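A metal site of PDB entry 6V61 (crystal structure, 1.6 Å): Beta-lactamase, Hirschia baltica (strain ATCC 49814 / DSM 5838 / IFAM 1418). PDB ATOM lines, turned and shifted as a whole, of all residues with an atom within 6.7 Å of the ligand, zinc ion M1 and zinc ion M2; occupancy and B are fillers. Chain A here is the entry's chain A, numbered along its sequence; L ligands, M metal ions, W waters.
Zinc ion M2 is bound by a ring nitrogen (NE2) of His 90 (2.0 Å), a ring nitrogen (NE2) of His 154 (2.0 Å), a ring nitrogen (ND1) of His 92 (2.1 Å) and a sulfur (S1) of the ligand (2.3 Å).
Zinc ion M2 has four donor atoms within binding distance.
Three residues have an atom within 4 Å of zinc ion M2: His 90, His 92 and His 154.
The nearest printed residue that does not touch zinc ion M2 is Cys 173 (4.1 Å).
Residues that only touch the ligand: Gly 184 (3.5 Å) and Ile 43 (3.6 Å).
Hydrophobic or aromatic side chains within 4 Å of the ligand: Ile 43, His 92, His 154 and His 215.
Of the 23 residues printed, 9 come within 4 Å of the ligand.
Along chain A the residues within 4 Å of the ligand span positions 43 to 215.
The nearest printed residue that does not touch the ligand is Trp 63 (4.1 Å).
O of Ile 43 is in hydrogen-bond range of NE1 of Trp 63, at 3.3 Å.
N of Ile 43 lies within hydrogen-bond range of O of Lys 35 (2.8 Å).
The backbone NH of Cys 173 lies within hydrogen-bond range of the side-chain hydroxyl of Ser 214 (3.2 Å).
The backbone carbonyl oxygen of Arg 44 lies within hydrogen-bond range of a ring nitrogen (ND1) of His 215 (2.7 Å).
The nearest printed residue that does not touch zinc ion M1 is His 90 (4.4 Å).
O2 of the ligand sits close to N of Asn 185, 3.5 Å away.
OD2 of Asp 94 binds zinc ion M1, 2.0 Å away.
A ring nitrogen (NE2) of His 215 binds zinc ion M1.
The side-chain sulfur (SG) of Cys 173 is bound to zinc ion M1.
S1 of the ligand binds zinc ion M1 (2.3 Å).
Zinc ion M1 has four donor atoms within binding distance.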
ATOM      1  N   LYS A  35       9.104  -7.876 -21.745  1.00  0.00           N
ATOM      2  CA  LYS A  35       8.714  -6.613 -22.346  1.00  0.00           C
ATOM      3  C   LYS A  35       7.669  -6.901 -23.394  1.00  0.00           C
ATOM      4  O   LYS A  35       7.821  -7.864 -24.159  1.00  0.00           O
ATOM      5  CB  LYS A  35       9.890  -5.885 -22.995  1.00  0.00           C
ATOM      6  CG  LYS A  35       9.533  -4.527 -23.592  1.00  0.00           C
ATOM      7  CD  LYS A  35      10.762  -3.894 -24.251  1.00  0.00           C
ATOM      8  CE  LYS A  35      10.440  -2.496 -24.764  1.00  0.00           C
ATOM      9  NZ  LYS A  35      11.661  -1.810 -25.290  1.00  0.00           N
ATOM     10  N   VAL A  37       6.297  -6.183 -26.779  1.00  0.00           N
ATOM     11  CA  VAL A  37       6.779  -5.613 -28.036  1.00  0.00           C
ATOM     12  C   VAL A  37       5.751  -5.910 -29.116  1.00  0.00           C
ATOM     13  O   VAL A  37       5.674  -7.033 -29.615  1.00  0.00           O
ATOM     14  CB  VAL A  37       8.153  -6.194 -28.402  1.00  0.00           C
ATOM     15  CG1 VAL A  37       8.646  -5.569 -29.712  1.00  0.00           C
ATOM     16  CG2 VAL A  37       9.147  -5.952 -27.266  1.00  0.00           C
ATOM     17  N   ILE A  43       7.982 -10.647 -24.598  1.00  0.00           N
ATOM     18  CA  ILE A  43       9.186 -11.374 -24.989  1.00  0.00           C
ATOM     19  C   ILE A  43      10.162 -11.351 -23.824  1.00  0.00           C
ATOM     20  O   ILE A  43      10.400 -10.298 -23.222  1.00  0.00           O
ATOM     21  CB  ILE A  43       9.822 -10.779 -26.265  1.00  0.00           C
ATOM     22  CG1 ILE A  43      11.163 -11.464 -26.560  1.00  0.00           C
ATOM     23  CG2 ILE A  43       9.983  -9.281 -26.149  1.00  0.00           C
ATOM     24  CD1 ILE A  43      11.040 -12.968 -26.745  1.00  0.00           C
ATOM     25  N   ARG A  44      10.717 -12.518 -23.513  1.00  0.00           N
ATOM     26  CA  ARG A  44      11.635 -12.683 -22.388  1.00  0.00           C
ATOM     27  C   ARG A  44      13.044 -12.273 -22.787  1.00  0.00           C
ATOM     28  O   ARG A  44      13.431 -12.346 -23.955  1.00  0.00           O
ATOM     29  CB  ARG A  44      11.686 -14.144 -21.911  1.00  0.00           C
ATOM     30  CG  ARG A  44      12.480 -15.067 -22.868  1.00  0.00           C
ATOM     31  CD  ARG A  44      12.360 -16.525 -22.491  1.00  0.00           C
ATOM     32  NE  ARG A  44      13.000 -16.811 -21.212  1.00  0.00           N
ATOM     33  CZ  ARG A  44      12.773 -17.920 -20.523  1.00  0.00           C
ATOM     34  NH1 ARG A  44      11.896 -18.834 -20.972  1.00  0.00           N
ATOM     35  NH2 ARG A  44      13.372 -18.114 -19.356  1.00  0.00           N
ATOM     36  N   THR A  45      13.807 -11.858 -21.790  1.00  0.00           N
ATOM     37  CA  THR A  45      15.259 -11.804 -21.914  1.00  0.00           C
ATOM     38  C   THR A  45      15.850 -12.414 -20.661  1.00  0.00           C
ATOM     39  O   THR A  45      15.345 -12.191 -19.559  1.00  0.00           O
ATOM     40  CB  THR A  45      15.786 -10.375 -22.147  1.00  0.00           C
ATOM     41  OG1 THR A  45      17.210 -10.424 -22.413  1.00  0.00           O
ATOM     42  CG2 THR A  45      15.562  -9.428 -20.927  1.00  0.00           C
ATOM     43  N   TRP A  63      15.314  -5.682 -18.956  1.00  0.00           N
ATOM     44  CA  TRP A  63      14.896  -4.714 -19.960  1.00  0.00           C
ATOM     45  C   TRP A  63      15.027  -3.276 -19.493  1.00  0.00           C
ATOM     46  O   TRP A  63      15.121  -2.362 -20.329  1.00  0.00           O
ATOM     47  CB  TRP A  63      13.447  -4.954 -20.374  1.00  0.00           C
ATOM     48  CG  TRP A  63      13.180  -6.228 -21.144  1.00  0.00           C
ATOM     49  CD1 TRP A  63      12.622  -7.377 -20.648  1.00  0.00           C
ATOM     50  CD2 TRP A  63      13.408  -6.459 -22.544  1.00  0.00           C
ATOM     51  NE1 TRP A  63      12.510  -8.315 -21.659  1.00  0.00           N
ATOM     52  CE2 TRP A  63      12.981  -7.775 -22.818  1.00  0.00           C
ATOM     53  CE3 TRP A  63      13.942  -5.682 -23.574  1.00  0.00           C
ATOM     54  CZ2 TRP A  63      13.060  -8.331 -24.106  1.00  0.00           C
ATOM     55  CZ3 TRP A  63      14.009  -6.231 -24.852  1.00  0.00           C
ATOM     56  CH2 TRP A  63      13.576  -7.545 -25.105  1.00  0.00           C
ATOM     57  N   HIS A  90      26.182  -7.425 -25.045  1.00  0.00           N
ATOM     58  CA  HIS A  90      26.247  -6.533 -26.215  1.00  0.00           C
ATOM     59  C   HIS A  90      25.365  -5.318 -25.946  1.00  0.00           C
ATOM     60  O   HIS A  90      24.613  -5.288 -24.960  1.00  0.00           O
ATOM     61  CB  HIS A  90      25.866  -7.201 -27.564  1.00  0.00           C
ATOM     62  CG  HIS A  90      24.435  -7.633 -27.679  1.00  0.00           C
ATOM     63  ND1 HIS A  90      23.942  -8.758 -27.061  1.00  0.00           N
ATOM     64  CD2 HIS A  90      23.386  -7.090 -28.352  1.00  0.00           C
ATOM     65  CE1 HIS A  90      22.661  -8.895 -27.344  1.00  0.00           C
ATOM     66  NE2 HIS A  90      22.292  -7.883 -28.122  1.00  0.00           N
ATOM     67  N   ALA A  91      25.444  -4.332 -26.848  1.00  0.00           N
ATOM     68  CA  ALA A  91      24.853  -3.006 -26.631  1.00  0.00           C
ATOM     69  C   ALA A  91      23.403  -2.914 -27.135  1.00  0.00           C
ATOM     70  O   ALA A  91      23.058  -2.064 -27.971  1.00  0.00           O
ATOM     71  CB  ALA A  91      25.714  -1.940 -27.288  1.00  0.00           C
ATOM     72  N   HIS A  92      22.535  -3.788 -26.626  1.00  0.00           N
ATOM     73  CA  HIS A  92      21.102  -3.649 -26.857  1.00  0.00           C
ATOM     74  C   HIS A  92      20.376  -3.516 -25.526  1.00  0.00           C
ATOM     75  O   HIS A  92      20.920  -3.842 -24.454  1.00  0.00           O
ATOM     76  CB  HIS A  92      20.518  -4.808 -27.673  1.00  0.00           C
ATOM     77  CG  HIS A  92      20.789  -4.718 -29.140  1.00  0.00           C
ATOM     78  ND1 HIS A  92      20.865  -5.848 -29.942  1.00  0.00           N
ATOM     79  CD2 HIS A  92      21.002  -3.663 -29.958  1.00  0.00           C
ATOM     80  CE1 HIS A  92      21.094  -5.483 -31.186  1.00  0.00           C
ATOM     81  NE2 HIS A  92      21.200  -4.155 -31.226  1.00  0.00           N
ATOM     82  N   SER A  93      19.124  -3.057 -25.600  1.00  0.00           N
ATOM     83  CA  SER A  93      18.426  -2.649 -24.383  1.00  0.00           C
ATOM     84  C   SER A  93      17.976  -3.833 -23.527  1.00  0.00           C
ATOM     85  O   SER A  93      17.673  -3.641 -22.338  1.00  0.00           O
ATOM     86  CB  SER A  93      17.227  -1.741 -24.729  1.00  0.00           C
ATOM     87  OG  SER A  93      16.154  -2.460 -25.320  1.00  0.00           O
ATOM     88  N   ASP A  94      17.946  -5.050 -24.061  1.00  0.00           N
ATOM     89  CA  ASP A  94      17.674  -6.184 -23.181  1.00  0.00           C
ATOM     90  C   ASP A  94      18.881  -6.564 -22.310  1.00  0.00           C
ATOM     91  O   ASP A  94      18.711  -7.272 -21.313  1.00  0.00           O
ATOM     92  CB  ASP A  94      17.191  -7.417 -23.983  1.00  0.00           C
ATOM     93  CG  ASP A  94      18.071  -7.774 -25.153  1.00  0.00           C
ATOM     94  OD1 ASP A  94      18.933  -6.988 -25.609  1.00  0.00           O
ATOM     95  OD2 ASP A  94      17.866  -8.902 -25.606  1.00  0.00           O
ATOM     96  N   LYS A  95      20.088  -6.127 -22.684  1.00  0.00           N
ATOM     97  CA  LYS A  95      21.310  -6.439 -21.950  1.00  0.00           C
ATOM     98  C   LYS A  95      21.854  -5.262 -21.174  1.00  0.00           C
ATOM     99  O   LYS A  95      22.614  -5.469 -20.220  1.00  0.00           O
ATOM    100  CB  LYS A  95      22.417  -6.904 -22.932  1.00  0.00           C
ATOM    101  CG  LYS A  95      21.927  -7.799 -24.071  1.00  0.00           C
ATOM    102  CD  LYS A  95      21.866  -9.271 -23.692  1.00  0.00           C
ATOM    103  CE  LYS A  95      20.621  -9.663 -22.882  1.00  0.00           C
ATOM    104  NZ  LYS A  95      20.764 -11.023 -22.266  1.00  0.00           N
ATOM    105  N   HIS A 154      25.125 -12.202 -33.911  1.00  0.00           N
ATOM    106  CA  HIS A 154      23.922 -11.415 -33.687  1.00  0.00           C
ATOM    107  C   HIS A 154      24.235  -9.930 -33.753  1.00  0.00           C
ATOM    108  O   HIS A 154      23.451  -9.124 -34.299  1.00  0.00           O
ATOM    109  CB  HIS A 154      23.331 -11.763 -32.329  1.00  0.00           C
ATOM    110  CG  HIS A 154      22.357 -10.735 -31.818  1.00  0.00           C
ATOM    111  ND1 HIS A 154      21.066 -10.639 -32.291  1.00  0.00           N
ATOM    112  CD2 HIS A 154      22.501  -9.756 -30.904  1.00  0.00           C
ATOM    113  CE1 HIS A 154      20.456  -9.644 -31.674  1.00  0.00           C
ATOM    114  NE2 HIS A 154      21.298  -9.094 -30.821  1.00  0.00           N
ATOM    115  N   SER A 155      25.374  -9.546 -33.199  1.00  0.00           N
ATOM    116  CA  SER A 155      25.878  -8.177 -33.261  1.00  0.00           C
ATOM    117  C   SER A 155      27.397  -8.221 -33.415  1.00  0.00           C
ATOM    118  O   SER A 155      28.030  -9.234 -33.117  1.00  0.00           O
ATOM    119  CB  SER A 155      25.507  -7.401 -32.012  1.00  0.00           C
ATOM    120  OG  SER A 155      26.149  -7.985 -30.902  1.00  0.00           O
ATOM    121  N   GLY A 172      23.784 -15.741 -24.724  1.00  0.00           N
ATOM    122  CA  GLY A 172      23.094 -14.476 -24.948  1.00  0.00           C
ATOM    123  C   GLY A 172      22.322 -14.511 -26.255  1.00  0.00           C
ATOM    124  O   GLY A 172      21.759 -15.544 -26.650  1.00  0.00           O
ATOM    125  N   CYS A 173      22.269 -13.367 -26.931  1.00  0.00           N
ATOM    126  CA  CYS A 173      21.405 -13.272 -28.101  1.00  0.00           C
ATOM    127  C   CYS A 173      22.071 -13.858 -29.333  1.00  0.00           C
ATOM    128  O   CYS A 173      21.405 -14.014 -30.361  1.00  0.00           O
ATOM    129  CB  CYS A 173      21.001 -11.818 -28.357  1.00  0.00           C
ATOM    130  SG  CYS A 173      20.252 -11.053 -26.874  1.00  0.00           S
ATOM    131  N   ARG A 176      20.146 -18.655 -30.775  1.00  0.00           N
ATOM    132  CA  ARG A 176      18.707 -18.594 -30.950  1.00  0.00           C
ATOM    133  C   ARG A 176      18.031 -19.704 -30.148  1.00  0.00           C
ATOM    134  O   ARG A 176      18.627 -20.754 -29.888  1.00  0.00           O
ATOM    135  CB  ARG A 176      18.354 -18.721 -32.428  1.00  0.00           C
ATOM    136  CG  ARG A 176      18.910 -17.561 -33.260  1.00  0.00           C
ATOM    137  CD  ARG A 176      18.222 -16.210 -32.940  1.00  0.00           C
ATOM    138  NE  ARG A 176      16.789 -16.270 -33.241  1.00  0.00           N
ATOM    139  CZ  ARG A 176      15.839 -15.661 -32.533  1.00  0.00           C
ATOM    140  NH1 ARG A 176      16.153 -14.941 -31.456  1.00  0.00           N
ATOM    141  NH2 ARG A 176      14.568 -15.799 -32.893  1.00  0.00           N
ATOM    142  N   LEU A 183      15.621 -15.541 -37.029  1.00  0.00           N
ATOM    143  CA  LEU A 183      16.910 -15.018 -36.607  1.00  0.00           C
ATOM    144  C   LEU A 183      16.784 -13.849 -35.636  1.00  0.00           C
ATOM    145  O   LEU A 183      17.804 -13.351 -35.164  1.00  0.00           O
ATOM    146  CB  LEU A 183      17.727 -14.575 -37.818  1.00  0.00           C
ATOM    147  CG  LEU A 183      17.992 -15.573 -38.945  1.00  0.00           C
ATOM    148  CD1 LEU A 183      19.177 -15.109 -39.767  1.00  0.00           C
ATOM    149  CD2 LEU A 183      18.252 -16.964 -38.393  1.00  0.00           C
ATOM    150  N   GLY A 184      15.557 -13.426 -35.320  1.00  0.00           N
ATOM    151  CA  GLY A 184      15.407 -12.242 -34.486  1.00  0.00           C
ATOM    152  C   GLY A 184      15.682 -11.008 -35.323  1.00  0.00           C
ATOM    153  O   GLY A 184      15.723 -11.038 -36.542  1.00  0.00           O
ATOM    154  N   ASN A 185      15.954  -9.901 -34.620  1.00  0.00           N
ATOM    155  CA  ASN A 185      16.275  -8.662 -35.315  1.00  0.00           C
ATOM    156  C   ASN A 185      17.718  -8.729 -35.820  1.00  0.00           C
ATOM    157  O   ASN A 185      18.646  -8.911 -35.015  1.00  0.00           O
ATOM    158  CB  ASN A 185      16.068  -7.452 -34.410  1.00  0.00           C
ATOM    159  CG  ASN A 185      16.211  -6.138 -35.143  1.00  0.00           C
ATOM    160  OD1 ASN A 185      17.219  -5.897 -35.810  1.00  0.00           O
ATOM    161  ND2 ASN A 185      15.198  -5.282 -35.043  1.00  0.00           N
ATOM    162  N   ILE A 186      17.894  -8.631 -37.123  1.00  0.00           N
ATOM    163  CA  ILE A 186      19.205  -8.801 -37.736  1.00  0.00           C
ATOM    164  C   ILE A 186      19.727  -7.502 -38.329  1.00  0.00           C
ATOM    165  O   ILE A 186      20.633  -7.520 -39.147  1.00  0.00           O
ATOM    166  CB  ILE A 186      19.189  -9.933 -38.783  1.00  0.00           C
ATOM    167  CG1 ILE A 186      18.107  -9.685 -39.838  1.00  0.00           C
ATOM    168  CG2 ILE A 186      18.974 -11.266 -38.104  1.00  0.00           C
ATOM    169  CD1 ILE A 186      18.319 -10.506 -41.100  1.00  0.00           C
ATOM    170  N   SER A 214      19.373 -15.784 -24.783  1.00  0.00           N
ATOM    171  CA  SER A 214      18.636 -14.696 -24.147  1.00  0.00           C
ATOM    172  C   SER A 214      17.125 -14.853 -24.288  1.00  0.00           C
ATOM    173  O   SER A 214      16.385 -14.462 -23.386  1.00  0.00           O
ATOM    174  CB  SER A 214      19.033 -13.330 -24.709  1.00  0.00           C
ATOM    175  OG  SER A 214      20.350 -12.998 -24.378  1.00  0.00           O
ATOM    176  N   HIS A 215      16.647 -15.360 -25.421  1.00  0.00           N
ATOM    177  CA  HIS A 215      15.232 -15.202 -25.751  1.00  0.00           C
ATOM    178  C   HIS A 215      14.468 -16.518 -25.821  1.00  0.00           C
ATOM    179  O   HIS A 215      13.470 -16.629 -26.520  1.00  0.00           O
ATOM    180  CB  HIS A 215      15.067 -14.411 -27.050  1.00  0.00           C
ATOM    181  CG  HIS A 215      15.627 -13.030 -26.965  1.00  0.00           C
ATOM    182  ND1 HIS A 215      15.199 -12.115 -26.016  1.00  0.00           N
ATOM    183  CD2 HIS A 215      16.620 -12.411 -27.651  1.00  0.00           C
ATOM    184  CE1 HIS A 215      15.881 -10.999 -26.136  1.00  0.00           C
ATOM    185  NE2 HIS A 215      16.745 -11.146 -27.134  1.00  0.00           N
HETATM  186  O1  LIG L   1      16.251  -6.955 -31.094  1.00  0.00           O
HETATM  187  C1  LIG L   1      15.754  -7.398 -30.061  1.00  0.00           C
HETATM  188  C2  LIG L   1      16.245  -6.893 -28.743  1.00  0.00           C
HETATM  189  C3  LIG L   1      17.770  -6.903 -28.745  1.00  0.00           C
HETATM  190  S1  LIG L   1      18.518  -8.512 -29.152  1.00  0.00           S
HETATM  191  C4  LIG L   1      15.714  -5.483 -28.471  1.00  0.00           C
HETATM  192  N1  LIG L   1      14.781  -8.317 -30.001  1.00  0.00           N
HETATM  193  C5  LIG L   1      14.771  -9.555 -30.774  1.00  0.00           C
HETATM  194  C6  LIG L   1      13.803  -9.546 -31.912  1.00  0.00           C
HETATM  195  O2  LIG L   1      13.572  -8.466 -32.503  1.00  0.00           O
HETATM  196  O3  LIG L   1      13.258 -10.641 -32.213  1.00  0.00           O
HETATM  197  C7  LIG L   1      13.627  -8.280 -29.109  1.00  0.00           C
HETATM  198  C8  LIG L   1      13.520  -9.748 -28.709  1.00  0.00           C
HETATM  199  C9  LIG L   1      14.227 -10.563 -29.785  1.00  0.00           C
HETATM  200 ZN    ZN M   1      18.400  -9.833 -27.272  1.00  0.00          ZN
HETATM  201 ZN    ZN M   2      20.730  -7.819 -29.352  1.00  0.00          ZN
HETATM  202  O   HOH W   1      12.531  -4.510 -29.530  1.00  0.00           O
HETATM  203  O   HOH W   2      17.473 -11.526 -31.176  1.00  0.00           O
HETATM  204  O   HOH W   3      13.368  -6.058 -31.634  1.00  0.00           O
HETATM  205  O   HOH W   4      13.572 -13.709 -30.493  1.00  0.00           O
